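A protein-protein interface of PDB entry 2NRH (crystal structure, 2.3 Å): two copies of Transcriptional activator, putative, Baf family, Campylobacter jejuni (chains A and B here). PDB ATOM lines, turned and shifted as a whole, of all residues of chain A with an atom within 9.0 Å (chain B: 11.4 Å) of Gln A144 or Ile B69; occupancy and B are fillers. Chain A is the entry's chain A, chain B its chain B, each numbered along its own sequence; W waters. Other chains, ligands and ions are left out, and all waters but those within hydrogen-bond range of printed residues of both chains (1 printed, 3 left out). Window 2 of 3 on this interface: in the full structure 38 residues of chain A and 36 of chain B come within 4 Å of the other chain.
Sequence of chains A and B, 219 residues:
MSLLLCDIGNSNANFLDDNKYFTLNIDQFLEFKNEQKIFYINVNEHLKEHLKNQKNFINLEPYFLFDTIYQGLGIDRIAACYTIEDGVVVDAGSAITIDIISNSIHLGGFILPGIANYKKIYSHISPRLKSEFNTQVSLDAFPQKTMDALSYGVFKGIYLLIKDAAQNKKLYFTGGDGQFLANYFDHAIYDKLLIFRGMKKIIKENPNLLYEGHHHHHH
The side-chain amide nitrogen (NE2) of Gln A144 lies within hydrogen-bond range of the backbone carbonyl oxygen (O) of Leu B107 (3.3 Å).
The backbone NH of Gln B71 is in hydrogen-bond range of the backbone carbonyl oxygen of Gln A144.
The backbone NH (N) of Gly B109 is in hydrogen-bond range of the backbone carbonyl oxygen (O) of Pro A143, 3.2 Å away.
The backbone carbonyl oxygen of Ala A149 lies within hydrogen-bond range of the backbone NH of Ile B111 (3.4 Å).
OH of Tyr B70 sits at hydrogen-bond distance from NH1 of Arg B77, 3.2 Å away.
A ring nitrogen (ND1) of His B106 lies within hydrogen-bond range of the side-chain hydroxyl (OG1) of Thr B68 (2.5 Å).
O of Ile B100 is in hydrogen-bond range of N of Leu B107, 2.8 Å away.
A ring nitrogen (NE2) of His B106 is in hydrogen-bond range of the backbone carbonyl oxygen (O) of Gly B108 (3.2 Å).
The backbone NH of His B106 sits at hydrogen-bond distance from the backbone carbonyl oxygen of Asp B67 (2.9 Å).
NE2 of His B106 lies within hydrogen-bond range of OD1 of Asp B99 (2.8 Å).
Ile B100 touches Phe A142.
Phe A142 touches Leu B107 (CB to O, 3.5 Å).
Gly B108 touches Phe A142.
O of Pro A143 touches CD1 of Tyr B70 (3.7 Å).
Gly B108 touches Pro A143 (CA to O, 3.2 Å).
Tyr B70 touches Gln A144.
OH of Tyr B70 touches C of Lys A145, at 3.8 Å.
Ala A149 touches Gly B109.
O of Ala A149 touches CB of Phe B110 (3.5 Å).
Ile B111 touches Leu A150 (CB to CD2, 3.9 Å).
Of chain B, only Ile B69, Tyr B70, Gln B71, His B106, Leu B107 and Gly B108 come within 4 Å of Gln A144.
Ile B69 touches one residue of chain A.
Pro A143 touches just these residues of chain B: Tyr B70, Gly B108 and Gly B109.
Of the printed residues of chain B, Lys A145 touches Tyr B70.
No residue of chain B comes within 4 Å of Asp A148.
No residue of chain A comes within 4 Å of Thr B68.
Of the printed residues of chain A, Leu B107 touches Phe A142 (3.5 Å) and Gln A144 (3.3 Å).
Of the printed residues of chain A, Gly B108 touches Phe A142 (3.6 Å), Pro A143 (3.2 Å) and Gln A144 (3.8 Å).
Printed residues of chain A within 4 Å of Gly B109: Pro A143 and Ala A149.
Printed residues of chain A within 4 Å of Ile B111: Ala A149 and Leu A150.
Of the printed residues of chain A, Gln B71 touches Gln A144 (3.0 Å).
The nearest residue of chain B that does not touch Gln A144 is Gly B109 (5.0 Å).
The nearest residue of chain A that does not touch Ile B69 is Lys A145 (6.0 Å).
Of the 25 printed residues of chain B, 10 touch a printed residue of chain A.
Hydrophobic or aromatic side chains of chain B that line the printed part of chain A: Ile B69, Tyr B70, Ile B100, Phe B110 and Ile B111.
Of the 13 printed residues of chain A, 8 touch a printed residue of chain B.
Hydrophobic or aromatic side chains of chain A that line the printed part of chain B: Phe A142, Pro A143, Ala A149, Leu A150 and Tyr A152.
Along chain A the printed residues that touch a printed residue of chain B span positions 142 to 152.
Among the printed residues, no Asp or Glu carboxylate lies within 4 Å of a Lys or Arg side-chain nitrogen of the other chain.
No position is printed for both chains.
Of the 20 pairs that touch across the chains among the printed residues, none has its exchanged pair printed and touching as well.
Water W1 bridges O of Gln B71 (2.7 Å) and N of Thr A146 (2.9 Å).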
ATOM      1  N   VAL A 137      15.106 -14.834 -23.048  1.00  0.00           N
ATOM      2  CA  VAL A 137      16.289 -14.891 -22.198  1.00  0.00           C
ATOM      3  C   VAL A 137      16.339 -16.261 -21.542  1.00  0.00           C
ATOM      4  O   VAL A 137      15.318 -16.777 -21.115  1.00  0.00           O
ATOM      5  CB  VAL A 137      16.346 -13.744 -21.108  1.00  0.00           C
ATOM      6  CG1 VAL A 137      15.040 -13.705 -20.195  1.00  0.00           C
ATOM      7  CG2 VAL A 137      17.614 -13.855 -20.259  1.00  0.00           C
ATOM      8  N   SER A 138      17.517 -16.860 -21.450  1.00  0.00           N
ATOM      9  CA  SER A 138      17.574 -18.083 -20.696  1.00  0.00           C
ATOM     10  C   SER A 138      17.448 -17.788 -19.208  1.00  0.00           C
ATOM     11  O   SER A 138      18.025 -16.821 -18.692  1.00  0.00           O
ATOM     12  CB  SER A 138      18.826 -18.920 -20.983  1.00  0.00           C
ATOM     13  OG  SER A 138      19.145 -19.739 -19.862  1.00  0.00           O
ATOM     14  N   ALA A 141      20.852 -19.794 -16.925  1.00  0.00           N
ATOM     15  CA  ALA A 141      22.191 -19.225 -16.906  1.00  0.00           C
ATOM     16  C   ALA A 141      22.105 -17.770 -16.470  1.00  0.00           C
ATOM     17  O   ALA A 141      21.079 -17.117 -16.730  1.00  0.00           O
ATOM     18  CB  ALA A 141      22.860 -19.321 -18.282  1.00  0.00           C
ATOM     19  N   PHE A 142      23.190 -17.306 -15.824  1.00  0.00           N
ATOM     20  CA  PHE A 142      23.367 -15.921 -15.395  1.00  0.00           C
ATOM     21  C   PHE A 142      23.581 -14.987 -16.565  1.00  0.00           C
ATOM     22  O   PHE A 142      24.434 -15.242 -17.420  1.00  0.00           O
ATOM     23  CB  PHE A 142      24.529 -15.823 -14.435  1.00  0.00           C
ATOM     24  CG  PHE A 142      24.298 -16.541 -13.170  1.00  0.00           C
ATOM     25  CD1 PHE A 142      23.046 -16.406 -12.481  1.00  0.00           C
ATOM     26  CD2 PHE A 142      25.302 -17.358 -12.627  1.00  0.00           C
ATOM     27  CE1 PHE A 142      22.802 -17.096 -11.293  1.00  0.00           C
ATOM     28  CE2 PHE A 142      25.088 -18.063 -11.434  1.00  0.00           C
ATOM     29  CZ  PHE A 142      23.825 -17.950 -10.758  1.00  0.00           C
ATOM     30  N   PRO A 143      22.777 -13.918 -16.653  1.00  0.00           N
ATOM     31  CA  PRO A 143      22.935 -12.969 -17.764  1.00  0.00           C
ATOM     32  C   PRO A 143      24.330 -12.331 -17.860  1.00  0.00           C
ATOM     33  O   PRO A 143      25.063 -12.237 -16.875  1.00  0.00           O
ATOM     34  CB  PRO A 143      21.949 -11.872 -17.411  1.00  0.00           C
ATOM     35  CG  PRO A 143      20.951 -12.523 -16.562  1.00  0.00           C
ATOM     36  CD  PRO A 143      21.672 -13.530 -15.760  1.00  0.00           C
ATOM     37  N   GLN A 144      24.634 -11.831 -19.045  1.00  0.00           N
ATOM     38  CA  GLN A 144      25.858 -11.134 -19.312  1.00  0.00           C
ATOM     39  C   GLN A 144      25.719  -9.867 -20.154  1.00  0.00           C
ATOM     40  O   GLN A 144      26.682  -9.358 -20.704  1.00  0.00           O
ATOM     41  CB  GLN A 144      26.904 -12.139 -19.858  1.00  0.00           C
ATOM     42  CG  GLN A 144      27.972 -12.367 -18.750  1.00  0.00           C
ATOM     43  CD  GLN A 144      28.087 -13.742 -18.358  1.00  0.00           C
ATOM     44  OE1 GLN A 144      27.140 -14.502 -18.503  1.00  0.00           O
ATOM     45  NE2 GLN A 144      29.271 -14.124 -17.831  1.00  0.00           N
ATOM     46  N   LYS A 145      24.514  -9.358 -20.283  1.00  0.00           N
ATOM     47  CA  LYS A 145      24.329  -7.963 -20.692  1.00  0.00           C
ATOM     48  C   LYS A 145      23.127  -7.341 -19.981  1.00  0.00           C
ATOM     49  O   LYS A 145      22.285  -8.050 -19.421  1.00  0.00           O
ATOM     50  CB  LYS A 145      24.199  -7.840 -22.192  1.00  0.00           C
ATOM     51  CG  LYS A 145      23.056  -8.572 -22.774  1.00  0.00           C
ATOM     52  CD  LYS A 145      23.506  -9.347 -23.978  1.00  0.00           C
ATOM     53  CE  LYS A 145      22.907  -8.799 -25.203  1.00  0.00           C
ATOM     54  NZ  LYS A 145      23.053  -9.854 -26.244  1.00  0.00           N
ATOM     55  N   THR A 146      23.097  -6.021 -19.947  1.00  0.00           N
ATOM     56  CA  THR A 146      22.041  -5.289 -19.245  1.00  0.00           C
ATOM     57  C   THR A 146      20.599  -5.707 -19.560  1.00  0.00           C
ATOM     58  O   THR A 146      19.831  -5.842 -18.636  1.00  0.00           O
ATOM     59  CB  THR A 146      22.207  -3.767 -19.398  1.00  0.00           C
ATOM     60  OG1 THR A 146      23.456  -3.419 -18.815  1.00  0.00           O
ATOM     61  CG2 THR A 146      21.099  -2.972 -18.624  1.00  0.00           C
ATOM     62  N   MET A 147      20.236  -5.909 -20.832  1.00  0.00           N
ATOM     63  CA  MET A 147      18.820  -6.193 -21.172  1.00  0.00           C
ATOM     64  C   MET A 147      18.375  -7.563 -20.696  1.00  0.00           C
ATOM     65  O   MET A 147      17.239  -7.745 -20.262  1.00  0.00           O
ATOM     66  CB  MET A 147      18.516  -6.038 -22.669  1.00  0.00           C
ATOM     67  CG  MET A 147      16.962  -6.144 -23.015  1.00  0.00           C
ATOM     68  SD  MET A 147      15.864  -4.972 -22.087  1.00  0.00           S
ATOM     69  CE  MET A 147      16.851  -3.446 -22.311  1.00  0.00           C
ATOM     70  N   ASP A 148      19.297  -8.508 -20.809  1.00  0.00           N
ATOM     71  CA  ASP A 148      19.191  -9.832 -20.225  1.00  0.00           C
ATOM     72  C   ASP A 148      19.184  -9.812 -18.685  1.00  0.00           C
ATOM     73  O   ASP A 148      18.415 -10.566 -18.075  1.00  0.00           O
ATOM     74  CB  ASP A 148      20.329 -10.738 -20.730  1.00  0.00           C
ATOM     75  CG  ASP A 148      20.161 -11.188 -22.223  1.00  0.00           C
ATOM     76  OD1 ASP A 148      21.016 -12.050 -22.585  1.00  0.00           O
ATOM     77  OD2 ASP A 148      19.290 -10.687 -23.037  1.00  0.00           O
ATOM     78  N   ALA A 149      20.059  -9.013 -18.071  1.00  0.00           N
ATOM     79  CA  ALA A 149      20.048  -8.845 -16.622  1.00  0.00           C
ATOM     80  C   ALA A 149      18.662  -8.375 -16.147  1.00  0.00           C
ATOM     81  O   ALA A 149      18.094  -8.929 -15.189  1.00  0.00           O
ATOM     82  CB  ALA A 149      21.162  -7.889 -16.150  1.00  0.00           C
ATOM     83  N   LEU A 150      18.072  -7.420 -16.867  1.00  0.00           N
ATOM     84  CA  LEU A 150      16.749  -6.922 -16.503  1.00  0.00           C
ATOM     85  C   LEU A 150      15.644  -7.974 -16.688  1.00  0.00           C
ATOM     86  O   LEU A 150      14.758  -8.140 -15.844  1.00  0.00           O
ATOM     87  CB  LEU A 150      16.438  -5.627 -17.267  1.00  0.00           C
ATOM     88  CG  LEU A 150      17.374  -4.440 -16.998  1.00  0.00           C
ATOM     89  CD1 LEU A 150      17.143  -3.293 -17.944  1.00  0.00           C
ATOM     90  CD2 LEU A 150      17.261  -3.929 -15.609  1.00  0.00           C
ATOM     91  N   TYR A 152      15.755 -11.205 -16.970  1.00  0.00           N
ATOM     92  CA  TYR A 152      15.850 -12.337 -16.096  1.00  0.00           C
ATOM     93  C   TYR A 152      15.367 -12.001 -14.654  1.00  0.00           C
ATOM     94  O   TYR A 152      14.688 -12.805 -14.070  1.00  0.00           O
ATOM     95  CB  TYR A 152      17.299 -12.864 -16.152  1.00  0.00           C
ATOM     96  CG  TYR A 152      17.721 -13.897 -15.147  1.00  0.00           C
ATOM     97  CD1 TYR A 152      18.107 -15.174 -15.557  1.00  0.00           C
ATOM     98  CD2 TYR A 152      17.795 -13.590 -13.785  1.00  0.00           C
ATOM     99  CE1 TYR A 152      18.527 -16.126 -14.624  1.00  0.00           C
ATOM    100  CE2 TYR A 152      18.182 -14.555 -12.837  1.00  0.00           C
ATOM    101  CZ  TYR A 152      18.567 -15.799 -13.276  1.00  0.00           C
ATOM    102  OH  TYR A 152      18.995 -16.716 -12.351  1.00  0.00           O
ATOM    103  N   LEU B  65      41.298  -4.956 -12.591  1.00  0.00           N
ATOM    104  CA  LEU B  65      41.291  -6.126 -13.487  1.00  0.00           C
ATOM    105  C   LEU B  65      40.379  -7.262 -12.953  1.00  0.00           C
ATOM    106  O   LEU B  65      40.587  -7.865 -11.880  1.00  0.00           O
ATOM    107  CB  LEU B  65      42.728  -6.580 -13.863  1.00  0.00           C
ATOM    108  CG  LEU B  65      43.764  -5.461 -14.213  1.00  0.00           C
ATOM    109  CD1 LEU B  65      45.018  -6.028 -14.738  1.00  0.00           C
ATOM    110  CD2 LEU B  65      43.253  -4.323 -15.176  1.00  0.00           C
ATOM    111  N   PHE B  66      39.350  -7.564 -13.721  1.00  0.00           N
ATOM    112  CA  PHE B  66      38.259  -8.330 -13.218  1.00  0.00           C
ATOM    113  C   PHE B  66      37.769  -9.200 -14.339  1.00  0.00           C
ATOM    114  O   PHE B  66      37.438  -8.710 -15.379  1.00  0.00           O
ATOM    115  CB  PHE B  66      37.183  -7.335 -12.725  1.00  0.00           C
ATOM    116  CG  PHE B  66      35.958  -7.976 -12.183  1.00  0.00           C
ATOM    117  CD1 PHE B  66      35.977  -8.605 -10.955  1.00  0.00           C
ATOM    118  CD2 PHE B  66      34.767  -7.909 -12.894  1.00  0.00           C
ATOM    119  CE1 PHE B  66      34.849  -9.189 -10.451  1.00  0.00           C
ATOM    120  CE2 PHE B  66      33.646  -8.451 -12.387  1.00  0.00           C
ATOM    121  CZ  PHE B  66      33.680  -9.126 -11.169  1.00  0.00           C
ATOM    122  N   ASP B  67      37.736 -10.506 -14.133  1.00  0.00           N
ATOM    123  CA  ASP B  67      37.447 -11.448 -15.224  1.00  0.00           C
ATOM    124  C   ASP B  67      35.934 -11.648 -15.431  1.00  0.00           C
ATOM    125  O   ASP B  67      35.309 -12.379 -14.716  1.00  0.00           O
ATOM    126  CB  ASP B  67      38.184 -12.784 -14.976  1.00  0.00           C
ATOM    127  CG  ASP B  67      38.230 -13.714 -16.220  1.00  0.00           C
ATOM    128  OD1 ASP B  67      37.490 -13.529 -17.228  1.00  0.00           O
ATOM    129  OD2 ASP B  67      39.066 -14.668 -16.181  1.00  0.00           O
ATOM    130  N   THR B  68      35.387 -10.954 -16.424  1.00  0.00           N
ATOM    131  CA  THR B  68      33.930 -10.931 -16.798  1.00  0.00           C
ATOM    132  C   THR B  68      33.760 -10.855 -18.346  1.00  0.00           C
ATOM    133  O   THR B  68      34.644 -10.361 -19.031  1.00  0.00           O
ATOM    134  CB  THR B  68      33.152  -9.686 -16.100  1.00  0.00           C
ATOM    135  OG1 THR B  68      31.744  -9.804 -16.332  1.00  0.00           O
ATOM    136  CG2 THR B  68      33.561  -8.373 -16.679  1.00  0.00           C
ATOM    137  N   ILE B  69      32.640 -11.318 -18.890  1.00  0.00           N
ATOM    138  CA  ILE B  69      32.286 -11.069 -20.311  1.00  0.00           C
ATOM    139  C   ILE B  69      30.974 -10.290 -20.428  1.00  0.00           C
ATOM    140  O   ILE B  69      30.345 -10.226 -21.516  1.00  0.00           O
ATOM    141  CB  ILE B  69      32.101 -12.372 -21.143  1.00  0.00           C
ATOM    142  CG1 ILE B  69      31.099 -13.311 -20.480  1.00  0.00           C
ATOM    143  CG2 ILE B  69      33.455 -13.017 -21.462  1.00  0.00           C
ATOM    144  CD1 ILE B  69      30.720 -14.479 -21.350  1.00  0.00           C
ATOM    145  N   TYR B  70      30.519  -9.812 -19.275  1.00  0.00           N
ATOM    146  CA  TYR B  70      29.294  -9.048 -19.128  1.00  0.00           C
ATOM    147  C   TYR B  70      29.572  -7.704 -19.716  1.00  0.00           C
ATOM    148  O   TYR B  70      30.343  -6.944 -19.160  1.00  0.00           O
ATOM    149  CB  TYR B  70      28.929  -8.901 -17.630  1.00  0.00           C
ATOM    150  CG  TYR B  70      27.592  -8.229 -17.309  1.00  0.00           C
ATOM    151  CD1 TYR B  70      26.617  -8.895 -16.549  1.00  0.00           C
ATOM    152  CD2 TYR B  70      27.312  -6.928 -17.743  1.00  0.00           C
ATOM    153  CE1 TYR B  70      25.406  -8.285 -16.234  1.00  0.00           C
ATOM    154  CE2 TYR B  70      26.136  -6.307 -17.444  1.00  0.00           C
ATOM    155  CZ  TYR B  70      25.183  -6.973 -16.681  1.00  0.00           C
ATOM    156  OH  TYR B  70      24.013  -6.326 -16.377  1.00  0.00           O
ATOM    157  N   GLN B  71      28.919  -7.409 -20.834  1.00  0.00           N
ATOM    158  CA  GLN B  71      29.133  -6.146 -21.549  1.00  0.00           C
ATOM    159  C   GLN B  71      28.834  -4.887 -20.720  1.00  0.00           C
ATOM    160  O   GLN B  71      27.744  -4.702 -20.206  1.00  0.00           O
ATOM    161  CB  GLN B  71      28.275  -6.109 -22.820  1.00  0.00           C
ATOM    162  CG  GLN B  71      28.381  -7.352 -23.713  1.00  0.00           C
ATOM    163  CD  GLN B  71      27.357  -7.332 -24.845  1.00  0.00           C
ATOM    164  OE1 GLN B  71      26.663  -6.315 -25.082  1.00  0.00           O
ATOM    165  NE2 GLN B  71      27.245  -8.458 -25.554  1.00  0.00           N
ATOM    166  N   GLY B  72      29.801  -4.016 -20.616  1.00  0.00           N
ATOM    167  CA  GLY B  72      29.591  -2.757 -19.925  1.00  0.00           C
ATOM    168  C   GLY B  72      29.325  -2.852 -18.427  1.00  0.00           C
ATOM    169  O   GLY B  72      28.770  -1.922 -17.860  1.00  0.00           O
ATOM    170  N   LEU B  73      29.728  -3.951 -17.770  1.00  0.00           N
ATOM    171  CA  LEU B  73      29.522  -4.095 -16.312  1.00  0.00           C
ATOM    172  C   LEU B  73      29.882  -2.791 -15.548  1.00  0.00           C
ATOM    173  O   LEU B  73      30.916  -2.162 -15.840  1.00  0.00           O
ATOM    174  CB  LEU B  73      30.342  -5.274 -15.808  1.00  0.00           C
ATOM    175  CG  LEU B  73      30.150  -5.667 -14.334  1.00  0.00           C
ATOM    176  CD1 LEU B  73      28.648  -5.889 -13.943  1.00  0.00           C
ATOM    177  CD2 LEU B  73      30.976  -6.903 -14.089  1.00  0.00           C
ATOM    178  N   GLY B  74      29.027  -2.342 -14.626  1.00  0.00           N
ATOM    179  CA  GLY B  74      29.263  -1.076 -13.930  1.00  0.00           C
ATOM    180  C   GLY B  74      30.454  -1.193 -12.998  1.00  0.00           C
ATOM    181  O   GLY B  74      30.662  -2.223 -12.332  1.00  0.00           O
ATOM    182  N   ARG B  77      29.617  -2.293  -9.430  1.00  0.00           N
ATOM    183  CA  ARG B  77      29.492  -3.750  -9.240  1.00  0.00           C
ATOM    184  C   ARG B  77      30.870  -4.432  -9.254  1.00  0.00           C
ATOM    185  O   ARG B  77      31.128  -5.305  -8.438  1.00  0.00           O
ATOM    186  CB  ARG B  77      28.576  -4.317 -10.317  1.00  0.00           C
ATOM    187  CG  ARG B  77      27.181  -3.730 -10.173  1.00  0.00           C
ATOM    188  CD  ARG B  77      26.243  -4.058 -11.339  1.00  0.00           C
ATOM    189  NE  ARG B  77      25.947  -5.464 -11.513  1.00  0.00           N
ATOM    190  CZ  ARG B  77      25.338  -5.976 -12.578  1.00  0.00           C
ATOM    191  NH1 ARG B  77      24.871  -5.198 -13.540  1.00  0.00           N
ATOM    192  NH2 ARG B  77      25.112  -7.271 -12.649  1.00  0.00           N
ATOM    193  N   ILE B  78      31.748  -4.035 -10.171  1.00  0.00           N
ATOM    194  CA  ILE B  78      33.091  -4.560 -10.183  1.00  0.00           C
ATOM    195  C   ILE B  78      33.773  -4.364  -8.804  1.00  0.00           C
ATOM    196  O   ILE B  78      34.247  -5.326  -8.208  1.00  0.00           O
ATOM    197  CB  ILE B  78      33.948  -3.967 -11.355  1.00  0.00           C
ATOM    198  CG1 ILE B  78      33.489  -4.556 -12.678  1.00  0.00           C
ATOM    199  CG2 ILE B  78      35.452  -4.264 -11.135  1.00  0.00           C
ATOM    200  CD1 ILE B  78      33.981  -3.868 -13.930  1.00  0.00           C
ATOM    201  N   ILE B  98      22.639  -8.392  -8.410  1.00  0.00           N
ATOM    202  CA  ILE B  98      23.097  -9.676  -7.854  1.00  0.00           C
ATOM    203  C   ILE B  98      24.176 -10.226  -8.776  1.00  0.00           C
ATOM    204  O   ILE B  98      23.939 -10.507  -9.930  1.00  0.00           O
ATOM    205  CB  ILE B  98      21.917 -10.681  -7.701  1.00  0.00           C
ATOM    206  CG1 ILE B  98      20.823 -10.152  -6.791  1.00  0.00           C
ATOM    207  CG2 ILE B  98      22.384 -11.977  -7.039  1.00  0.00           C
ATOM    208  CD1 ILE B  98      19.643  -9.554  -7.471  1.00  0.00           C
ATOM    209  N   ASP B  99      25.386 -10.344  -8.287  1.00  0.00           N
ATOM    210  CA  ASP B  99      26.506 -10.851  -9.114  1.00  0.00           C
ATOM    211  C   ASP B  99      27.123 -12.133  -8.538  1.00  0.00           C
ATOM    212  O   ASP B  99      27.270 -12.309  -7.318  1.00  0.00           O
ATOM    213  CB  ASP B  99      27.568  -9.770  -9.279  1.00  0.00           C
ATOM    214  CG  ASP B  99      27.119  -8.635 -10.225  1.00  0.00           C
ATOM    215  OD1 ASP B  99      27.026  -8.911 -11.454  1.00  0.00           O
ATOM    216  OD2 ASP B  99      26.872  -7.488  -9.725  1.00  0.00           O
ATOM    217  N   ILE B 100      27.521 -13.021  -9.427  1.00  0.00           N
ATOM    218  CA  ILE B 100      28.010 -14.325  -8.996  1.00  0.00           C
ATOM    219  C   ILE B 100      29.486 -14.528  -9.276  1.00  0.00           C
ATOM    220  O   ILE B 100      29.912 -14.480 -10.425  1.00  0.00           O
ATOM    221  CB  ILE B 100      27.140 -15.483  -9.572  1.00  0.00           C
ATOM    222  CG1 ILE B 100      25.658 -15.332  -9.104  1.00  0.00           C
ATOM    223  CG2 ILE B 100      27.694 -16.847  -9.094  1.00  0.00           C
ATOM    224  CD1 ILE B 100      24.854 -14.248  -9.786  1.00  0.00           C
ATOM    225  N   ILE B 101      30.258 -14.727  -8.199  1.00  0.00           N
ATOM    226  CA  ILE B 101      31.695 -14.960  -8.282  1.00  0.00           C
ATOM    227  C   ILE B 101      32.065 -16.416  -7.907  1.00  0.00           C
ATOM    228  O   ILE B 101      31.555 -17.029  -6.933  1.00  0.00           O
ATOM    229  CB  ILE B 101      32.491 -13.949  -7.410  1.00  0.00           C
ATOM    230  CG1 ILE B 101      31.932 -12.499  -7.567  1.00  0.00           C
ATOM    231  CG2 ILE B 101      34.017 -14.013  -7.697  1.00  0.00           C
ATOM    232  CD1 ILE B 101      32.109 -11.839  -8.958  1.00  0.00           C
ATOM    233  N   SER B 102      32.940 -16.982  -8.728  1.00  0.00           N
ATOM    234  CA  SER B 102      33.421 -18.321  -8.498  1.00  0.00           C
ATOM    235  C   SER B 102      34.842 -18.309  -8.919  1.00  0.00           C
ATOM    236  O   SER B 102      35.142 -18.130 -10.082  1.00  0.00           O
ATOM    237  CB  SER B 102      32.665 -19.353  -9.298  1.00  0.00           C
ATOM    238  OG  SER B 102      33.247 -20.629  -9.065  1.00  0.00           O
ATOM    239  N   SER B 104      37.269 -16.162  -8.329  1.00  0.00           N
ATOM    240  CA  SER B 104      37.646 -14.890  -8.839  1.00  0.00           C
ATOM    241  C   SER B 104      37.188 -14.710 -10.292  1.00  0.00           C
ATOM    242  O   SER B 104      37.798 -13.910 -11.022  1.00  0.00           O
ATOM    243  CB  SER B 104      39.204 -14.700  -8.762  1.00  0.00           C
ATOM    244  OG  SER B 104      39.714 -14.590  -7.433  1.00  0.00           O
ATOM    245  N   ILE B 105      36.174 -15.451 -10.737  1.00  0.00           N
ATOM    246  CA  ILE B 105      35.562 -15.213 -12.070  1.00  0.00           C
ATOM    247  C   ILE B 105      34.108 -14.791 -11.953  1.00  0.00           C
ATOM    248  O   ILE B 105      33.357 -15.334 -11.150  1.00  0.00           O
ATOM    249  CB  ILE B 105      35.707 -16.437 -13.007  1.00  0.00           C
ATOM    250  CG1 ILE B 105      37.206 -16.700 -13.269  1.00  0.00           C
ATOM    251  CG2 ILE B 105      35.061 -16.178 -14.401  1.00  0.00           C
ATOM    252  CD1 ILE B 105      37.518 -18.073 -13.749  1.00  0.00           C
ATOM    253  N   HIS B 106      33.718 -13.798 -12.741  1.00  0.00           N
ATOM    254  CA  HIS B 106      32.366 -13.232 -12.729  1.00  0.00           C
ATOM    255  C   HIS B 106      31.569 -14.066 -13.696  1.00  0.00           C
ATOM    256  O   HIS B 106      31.838 -14.079 -14.900  1.00  0.00           O
ATOM    257  CB  HIS B 106      32.395 -11.737 -13.133  1.00  0.00           C
ATOM    258  CG  HIS B 106      31.034 -11.086 -13.181  1.00  0.00           C
ATOM    259  ND1 HIS B 106      30.503 -10.548 -14.337  1.00  0.00           N
ATOM    260  CD2 HIS B 106      30.085 -10.928 -12.231  1.00  0.00           C
ATOM    261  CE1 HIS B 106      29.285 -10.092 -14.096  1.00  0.00           C
ATOM    262  NE2 HIS B 106      29.007 -10.312 -12.828  1.00  0.00           N
ATOM    263  N   LEU B 107      30.639 -14.834 -13.137  1.00  0.00           N
ATOM    264  CA  LEU B 107      29.830 -15.765 -13.871  1.00  0.00           C
ATOM    265  C   LEU B 107      28.602 -15.084 -14.516  1.00  0.00           C
ATOM    266  O   LEU B 107      27.875 -15.685 -15.316  1.00  0.00           O
ATOM    267  CB  LEU B 107      29.375 -16.881 -12.917  1.00  0.00           C
ATOM    268  CG  LEU B 107      30.433 -17.803 -12.255  1.00  0.00           C
ATOM    269  CD1 LEU B 107      29.750 -18.860 -11.394  1.00  0.00           C
ATOM    270  CD2 LEU B 107      31.396 -18.497 -13.212  1.00  0.00           C
ATOM    271  N   GLY B 108      28.325 -13.832 -14.183  1.00  0.00           N
ATOM    272  CA  GLY B 108      27.059 -13.289 -14.654  1.00  0.00           C
ATOM    273  C   GLY B 108      26.402 -12.609 -13.489  1.00  0.00           C
ATOM    274  O   GLY B 108      26.926 -12.642 -12.384  1.00  0.00           O
ATOM    275  N   GLY B 109      25.298 -11.942 -13.743  1.00  0.00           N
ATOM    276  CA  GLY B 109      24.616 -11.196 -12.682  1.00  0.00           C
ATOM    277  C   GLY B 109      23.287 -10.672 -13.196  1.00  0.00           C
ATOM    278  O   GLY B 109      22.997 -10.740 -14.421  1.00  0.00           O
ATOM    279  N   PHE B 110      22.472 -10.146 -12.290  1.00  0.00           N
ATOM    280  CA  PHE B 110      21.185  -9.588 -12.721  1.00  0.00           C
ATOM    281  C   PHE B 110      20.671  -8.489 -11.829  1.00  0.00           C
ATOM    282  O   PHE B 110      21.208  -8.252 -10.745  1.00  0.00           O
ATOM    283  CB  PHE B 110      20.119 -10.660 -12.901  1.00  0.00           C
ATOM    284  CG  PHE B 110      19.885 -11.488 -11.680  1.00  0.00           C
ATOM    285  CD1 PHE B 110      18.773 -11.223 -10.855  1.00  0.00           C
ATOM    286  CD2 PHE B 110      20.761 -12.548 -11.356  1.00  0.00           C
ATOM    287  CE1 PHE B 110      18.545 -11.988  -9.697  1.00  0.00           C
ATOM    288  CE2 PHE B 110      20.529 -13.349 -10.214  1.00  0.00           C
ATOM    289  CZ  PHE B 110      19.425 -13.077  -9.362  1.00  0.00           C
ATOM    290  N   ILE B 111      19.600  -7.858 -12.306  1.00  0.00           N
ATOM    291  CA  ILE B 111      19.136  -6.582 -11.761  1.00  0.00           C
ATOM    292  C   ILE B 111      17.644  -6.613 -11.456  1.00  0.00           C
ATOM    293  O   ILE B 111      16.760  -7.190 -12.201  1.00  0.00           O
ATOM    294  CB  ILE B 111      19.475  -5.349 -12.724  1.00  0.00           C
ATOM    295  CG1 ILE B 111      20.932  -5.375 -13.161  1.00  0.00           C
ATOM    296  CG2 ILE B 111      19.076  -3.986 -12.107  1.00  0.00           C
ATOM    297  CD1 ILE B 111      21.170  -4.523 -14.356  1.00  0.00           C
HETATM  298  O   HOH W   1      25.327  -4.930 -21.354  1.00  0.00           O
